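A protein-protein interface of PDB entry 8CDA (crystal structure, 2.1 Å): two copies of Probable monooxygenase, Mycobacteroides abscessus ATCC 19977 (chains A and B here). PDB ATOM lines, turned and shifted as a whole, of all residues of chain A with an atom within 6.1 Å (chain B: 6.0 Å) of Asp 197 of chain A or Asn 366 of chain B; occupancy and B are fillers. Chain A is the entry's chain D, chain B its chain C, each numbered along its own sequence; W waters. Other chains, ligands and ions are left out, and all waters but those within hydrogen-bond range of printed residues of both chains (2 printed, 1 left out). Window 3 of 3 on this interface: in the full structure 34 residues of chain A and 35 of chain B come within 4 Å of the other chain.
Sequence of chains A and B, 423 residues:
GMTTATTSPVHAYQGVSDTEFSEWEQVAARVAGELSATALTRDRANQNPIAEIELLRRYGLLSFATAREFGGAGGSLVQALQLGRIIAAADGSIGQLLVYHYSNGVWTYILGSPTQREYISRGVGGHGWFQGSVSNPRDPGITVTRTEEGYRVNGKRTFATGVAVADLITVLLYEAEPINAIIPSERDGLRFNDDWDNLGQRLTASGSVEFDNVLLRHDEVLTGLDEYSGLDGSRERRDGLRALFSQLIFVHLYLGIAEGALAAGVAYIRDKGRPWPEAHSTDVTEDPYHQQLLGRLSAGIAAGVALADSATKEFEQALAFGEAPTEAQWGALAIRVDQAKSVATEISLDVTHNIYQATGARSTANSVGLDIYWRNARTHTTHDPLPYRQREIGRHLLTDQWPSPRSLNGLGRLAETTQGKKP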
ATOM      1  N   ASN A  46      10.234  35.326 -24.432  1.00  0.00           N
ATOM      2  CA  ASN A  46      11.645  35.504 -24.079  1.00  0.00           C
ATOM      3  C   ASN A  46      12.063  36.975 -24.070  1.00  0.00           C
ATOM      4  O   ASN A  46      13.213  37.307 -24.366  1.00  0.00           O
ATOM      5  CB  ASN A  46      12.567  34.665 -24.973  1.00  0.00           C
ATOM      6  CG  ASN A  46      13.924  34.415 -24.343  1.00  0.00           C
ATOM      7  OD1 ASN A  46      14.062  34.405 -23.119  1.00  0.00           O
ATOM      8  ND2 ASN A  46      14.936  34.216 -25.180  1.00  0.00           N
ATOM      9  N   ASP A 195      21.842  37.029 -26.029  1.00  0.00           N
ATOM     10  CA  ASP A 195      22.238  35.635 -26.192  1.00  0.00           C
ATOM     11  C   ASP A 195      21.603  34.712 -25.159  1.00  0.00           C
ATOM     12  O   ASP A 195      22.051  33.568 -25.010  1.00  0.00           O
ATOM     13  CB  ASP A 195      23.763  35.496 -26.165  1.00  0.00           C
ATOM     14  CG  ASP A 195      24.383  36.089 -24.913  1.00  0.00           C
ATOM     15  OD1 ASP A 195      23.645  36.700 -24.112  1.00  0.00           O
ATOM     16  OD2 ASP A 195      25.610  35.946 -24.731  1.00  0.00           O
ATOM     17  N   TRP A 196      20.580  35.170 -24.444  1.00  0.00           N
ATOM     18  CA  TRP A 196      19.927  34.356 -23.422  1.00  0.00           C
ATOM     19  C   TRP A 196      18.740  33.650 -24.064  1.00  0.00           C
ATOM     20  O   TRP A 196      17.661  34.229 -24.214  1.00  0.00           O
ATOM     21  CB  TRP A 196      19.508  35.219 -22.235  1.00  0.00           C
ATOM     22  CG  TRP A 196      18.900  34.448 -21.100  1.00  0.00           C
ATOM     23  CD1 TRP A 196      17.637  34.584 -20.604  1.00  0.00           C
ATOM     24  CD2 TRP A 196      19.528  33.421 -20.317  1.00  0.00           C
ATOM     25  NE1 TRP A 196      17.438  33.711 -19.561  1.00  0.00           N
ATOM     26  CE2 TRP A 196      18.584  32.984 -19.366  1.00  0.00           C
ATOM     27  CE3 TRP A 196      20.796  32.830 -20.330  1.00  0.00           C
ATOM     28  CZ2 TRP A 196      18.867  31.986 -18.437  1.00  0.00           C
ATOM     29  CZ3 TRP A 196      21.075  31.838 -19.407  1.00  0.00           C
ATOM     30  CH2 TRP A 196      20.114  31.425 -18.473  1.00  0.00           C
ATOM     31  N   ASP A 197      18.950  32.394 -24.460  1.00  0.00           N
ATOM     32  CA  ASP A 197      17.908  31.529 -25.018  1.00  0.00           C
ATOM     33  C   ASP A 197      18.077  30.191 -24.310  1.00  0.00           C
ATOM     34  O   ASP A 197      18.721  29.273 -24.820  1.00  0.00           O
ATOM     35  CB  ASP A 197      18.047  31.400 -26.540  1.00  0.00           C
ATOM     36  CG  ASP A 197      16.947  30.558 -27.158  1.00  0.00           C
ATOM     37  OD1 ASP A 197      15.912  30.345 -26.492  1.00  0.00           O
ATOM     38  OD2 ASP A 197      17.120  30.097 -28.306  1.00  0.00           O
ATOM     39  N   ASN A 198      17.501  30.086 -23.121  1.00  0.00           N
ATOM     40  CA  ASN A 198      17.795  28.986 -22.219  1.00  0.00           C
ATOM     41  C   ASN A 198      16.586  28.074 -22.059  1.00  0.00           C
ATOM     42  O   ASN A 198      15.468  28.392 -22.473  1.00  0.00           O
ATOM     43  CB  ASN A 198      18.248  29.521 -20.856  1.00  0.00           C
ATOM     44  CG  ASN A 198      19.266  28.626 -20.195  1.00  0.00           C
ATOM     45  OD1 ASN A 198      20.417  28.559 -20.625  1.00  0.00           O
ATOM     46  ND2 ASN A 198      18.853  27.936 -19.138  1.00  0.00           N
ATOM     47  N   LEU A 199      16.838  26.916 -21.446  1.00  0.00           N
ATOM     48  CA  LEU A 199      15.768  25.970 -21.158  1.00  0.00           C
ATOM     49  C   LEU A 199      14.754  26.583 -20.202  1.00  0.00           C
ATOM     50  O   LEU A 199      13.567  26.714 -20.526  1.00  0.00           O
ATOM     51  CB  LEU A 199      16.366  24.696 -20.561  1.00  0.00           C
ATOM     52  CG  LEU A 199      15.367  23.689 -19.991  1.00  0.00           C
ATOM     53  CD1 LEU A 199      14.536  23.111 -21.123  1.00  0.00           C
ATOM     54  CD2 LEU A 199      16.081  22.592 -19.216  1.00  0.00           C
ATOM     55  N   GLY A 200      15.210  26.963 -19.014  1.00  0.00           N
ATOM     56  CA  GLY A 200      14.365  27.618 -18.039  1.00  0.00           C
ATOM     57  C   GLY A 200      14.982  28.917 -17.571  1.00  0.00           C
ATOM     58  O   GLY A 200      16.012  29.341 -18.107  1.00  0.00           O
ATOM     59  N   ARG A 202      14.074  31.778 -18.207  1.00  0.00           N
ATOM     60  CA  ARG A 202      14.266  32.506 -19.460  1.00  0.00           C
ATOM     61  C   ARG A 202      14.085  34.009 -19.292  1.00  0.00           C
ATOM     62  O   ARG A 202      14.685  34.788 -20.040  1.00  0.00           O
ATOM     63  CB  ARG A 202      13.316  31.967 -20.530  1.00  0.00           C
ATOM     64  CG  ARG A 202      13.594  30.531 -20.928  1.00  0.00           C
ATOM     65  CD  ARG A 202      12.429  29.916 -21.684  1.00  0.00           C
ATOM     66  NE  ARG A 202      12.012  30.712 -22.831  1.00  0.00           N
ATOM     67  CZ  ARG A 202      12.605  30.690 -24.018  1.00  0.00           C
ATOM     68  NH1 ARG A 202      13.684  29.958 -24.240  1.00  0.00           N
ATOM     69  NH2 ARG A 202      12.103  31.422 -25.008  1.00  0.00           N
ATOM     70  N   LEU B  40      17.218  19.007 -33.272  1.00  0.00           N
ATOM     71  CA  LEU B  40      16.776  20.217 -32.581  1.00  0.00           C
ATOM     72  C   LEU B  40      16.052  21.166 -33.527  1.00  0.00           C
ATOM     73  O   LEU B  40      14.963  21.659 -33.213  1.00  0.00           O
ATOM     74  CB  LEU B  40      17.965  20.918 -31.927  1.00  0.00           C
ATOM     75  CG  LEU B  40      18.602  20.199 -30.741  1.00  0.00           C
ATOM     76  CD1 LEU B  40      19.734  21.040 -30.172  1.00  0.00           C
ATOM     77  CD2 LEU B  40      17.553  19.903 -29.677  1.00  0.00           C
ATOM     78  N   ARG B  44      11.881  22.126 -33.157  1.00  0.00           N
ATOM     79  CA  ARG B  44      11.316  23.449 -32.919  1.00  0.00           C
ATOM     80  C   ARG B  44      10.424  23.899 -34.067  1.00  0.00           C
ATOM     81  O   ARG B  44       9.499  24.690 -33.855  1.00  0.00           O
ATOM     82  CB  ARG B  44      12.432  24.459 -32.650  1.00  0.00           C
ATOM     83  CG  ARG B  44      13.440  23.959 -31.626  1.00  0.00           C
ATOM     84  CD  ARG B  44      14.255  25.075 -31.001  1.00  0.00           C
ATOM     85  NE  ARG B  44      15.269  24.545 -30.095  1.00  0.00           N
ATOM     86  CZ  ARG B  44      15.046  24.196 -28.835  1.00  0.00           C
ATOM     87  NH1 ARG B  44      13.848  24.308 -28.285  1.00  0.00           N
ATOM     88  NH2 ARG B  44      16.052  23.719 -28.106  1.00  0.00           N
ATOM     89  N   SER B 363      25.110  23.714 -20.123  1.00  0.00           N
ATOM     90  CA  SER B 363      24.393  22.762 -20.966  1.00  0.00           C
ATOM     91  C   SER B 363      22.902  23.055 -21.057  1.00  0.00           C
ATOM     92  O   SER B 363      22.236  22.498 -21.937  1.00  0.00           O
ATOM     93  CB  SER B 363      24.608  21.329 -20.475  1.00  0.00           C
ATOM     94  OG  SER B 363      23.930  21.094 -19.250  1.00  0.00           O
ATOM     95  N   THR B 364      22.366  23.910 -20.184  1.00  0.00           N
ATOM     96  CA  THR B 364      20.947  24.248 -20.211  1.00  0.00           C
ATOM     97  C   THR B 364      20.585  25.232 -21.318  1.00  0.00           C
ATOM     98  O   THR B 364      19.403  25.562 -21.466  1.00  0.00           O
ATOM     99  CB  THR B 364      20.489  24.779 -18.845  1.00  0.00           C
ATOM    100  OG1 THR B 364      21.093  26.054 -18.587  1.00  0.00           O
ATOM    101  CG2 THR B 364      20.878  23.806 -17.737  1.00  0.00           C
ATOM    102  N   ALA B 365      21.558  25.703 -22.096  1.00  0.00           N
ATOM    103  CA  ALA B 365      21.254  26.566 -23.229  1.00  0.00           C
ATOM    104  C   ALA B 365      20.472  25.791 -24.280  1.00  0.00           C
ATOM    105  O   ALA B 365      20.729  24.608 -24.519  1.00  0.00           O
ATOM    106  CB  ALA B 365      22.546  27.103 -23.844  1.00  0.00           C
ATOM    107  N   ASN B 366      19.505  26.463 -24.908  1.00  0.00           N
ATOM    108  CA  ASN B 366      18.697  25.810 -25.932  1.00  0.00           C
ATOM    109  C   ASN B 366      19.505  25.439 -27.169  1.00  0.00           C
ATOM    110  O   ASN B 366      19.081  24.555 -27.923  1.00  0.00           O
ATOM    111  CB  ASN B 366      17.485  26.667 -26.304  1.00  0.00           C
ATOM    112  CG  ASN B 366      16.341  26.512 -25.323  1.00  0.00           C
ATOM    113  OD1 ASN B 366      16.192  25.470 -24.685  1.00  0.00           O
ATOM    114  ND2 ASN B 366      15.524  27.551 -25.197  1.00  0.00           N
ATOM    115  N   SER B 367      20.655  26.081 -27.395  1.00  0.00           N
ATOM    116  CA  SER B 367      21.518  25.660 -28.495  1.00  0.00           C
ATOM    117  C   SER B 367      22.111  24.282 -28.234  1.00  0.00           C
ATOM    118  O   SER B 367      22.492  23.581 -29.178  1.00  0.00           O
ATOM    119  CB  SER B 367      22.628  26.685 -28.726  1.00  0.00           C
ATOM    120  OG  SER B 367      23.431  26.832 -27.569  1.00  0.00           O
ATOM    121  N   VAL B 368      22.209  23.887 -26.966  1.00  0.00           N
ATOM    122  CA  VAL B 368      22.616  22.527 -26.633  1.00  0.00           C
ATOM    123  C   VAL B 368      21.434  21.572 -26.760  1.00  0.00           C
ATOM    124  O   VAL B 368      21.526  20.528 -27.417  1.00  0.00           O
ATOM    125  CB  VAL B 368      23.250  22.493 -25.230  1.00  0.00           C
ATOM    126  CG1 VAL B 368      23.621  21.073 -24.840  1.00  0.00           C
ATOM    127  CG2 VAL B 368      24.470  23.401 -25.185  1.00  0.00           C
ATOM    128  N   GLY B 369      20.309  21.916 -26.141  1.00  0.00           N
ATOM    129  CA  GLY B 369      19.083  21.157 -26.322  1.00  0.00           C
ATOM    130  C   GLY B 369      19.095  19.766 -25.728  1.00  0.00           C
ATOM    131  O   GLY B 369      18.536  18.837 -26.324  1.00  0.00           O
ATOM    132  N   ASP B 371      17.397  18.829 -23.292  1.00  0.00           N
ATOM    133  CA  ASP B 371      16.080  18.544 -22.739  1.00  0.00           C
ATOM    134  C   ASP B 371      15.166  17.808 -23.705  1.00  0.00           C
ATOM    135  O   ASP B 371      14.123  17.308 -23.271  1.00  0.00           O
ATOM    136  CB  ASP B 371      15.395  19.846 -22.331  1.00  0.00           C
ATOM    137  CG  ASP B 371      15.166  20.772 -23.510  1.00  0.00           C
ATOM    138  OD1 ASP B 371      16.143  21.065 -24.231  1.00  0.00           O
ATOM    139  OD2 ASP B 371      14.010  21.195 -23.723  1.00  0.00           O
HETATM  140  O   HOH W   1      19.715  28.837 -29.166  1.00  0.00           O
HETATM  141  O   HOH W   2      22.851  28.055 -19.805  1.00  0.00           O
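No position is printed for both chains.
Of the 9 pairs that touch across the chains among the printed residues, none has its exchanged pair printed and touching as well.
NH2 of Arg 44 of chain B lies within hydrogen-bond range of O of Asn 366 of chain B.
The backbone carbonyl oxygen (O) of Arg 202 of chain A lies close to the side-chain amide oxygen (OD1) of Asn 46 of chain A, 3.2 Å away.
O of Arg 202 of chain A lies within hydrogen-bond range of NE1 of Trp 196 of chain A (3.0 Å).
The guanidinium group (NH1) of Arg 202 of chain A is in salt-bridge range of the side-chain carboxylate (OD1) of Asp 197 of chain A.
ND2 of Asn 198 of chain A is in hydrogen-bond range of O of Gly 200 of chain A (3.3 Å).
The backbone carbonyl oxygen of Asn 198 of chain A lies within hydrogen-bond range of the guanidinium group of Arg 202 of chain A (3.0 Å).
Asp 197 of chain A touches just these residues of chain B: Ala 365 and Asn 366.
Of the printed residues of chain B, Arg 202 of chain A touches Asn 366 (3.2 Å).
Leu 40 of chain B touches none of the printed residues of chain A.
Of the printed residues of chain A, Ala 365 of chain B touches Asp 197 (3.9 Å) and Asn 198 (3.4 Å).
Of chain A, only Asp 197, Asn 198, Leu 199 and Arg 202 come within 4 Å of Asn 366 of chain B.
Among the printed residues, pairs that only touch across the chains: Asp 197 of chain A with Ala 365 of chain B, Leu 199 of chain A with Asn 366 of chain B and Leu 199 of chain A with Asp 371 of chain B.
Of the 10 printed residues of chain B, 4 touch a printed residue of chain A.
Among the printed residues, 9 pairs touch across the chains.
Water W2 bridges the side-chain amide oxygen of Asn 198 of chain A (2.6 Å) and the side-chain hydroxyl of Thr 364 of chain B (2.9 Å).
Water W1 lies within hydrogen-bond range of OD2 of Asp 197 of chain A (3.0 Å) and N of Ser 367 of chain B (3.4 Å).
ND2 of Asn 198 of chain A is in hydrogen-bond range of OG1 of Thr 364 of chain B (3.0 Å).
N of Leu 199 of chain A is in hydrogen-bond range of O of Thr 364 of chain B, at 2.9 Å.
The backbone NH of Ala 365 of chain B lies close to the side-chain amide oxygen of Asn 198 of chain A (3.4 Å).
The backbone NH of Asn 366 of chain B is in hydrogen-bond range of the backbone carbonyl oxygen of Asp 197 of chain A, 2.9 Å away.
The side-chain amide nitrogen (ND2) of Asn 366 of chain B is in hydrogen-bond range of the backbone carbonyl oxygen (O) of Asn 198 of chain A, at 2.9 Å.
The guanidinium group of Arg 202 of chain A lies close to the side-chain amide nitrogen of Asn 366 of chain B, 3.2 Å away.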
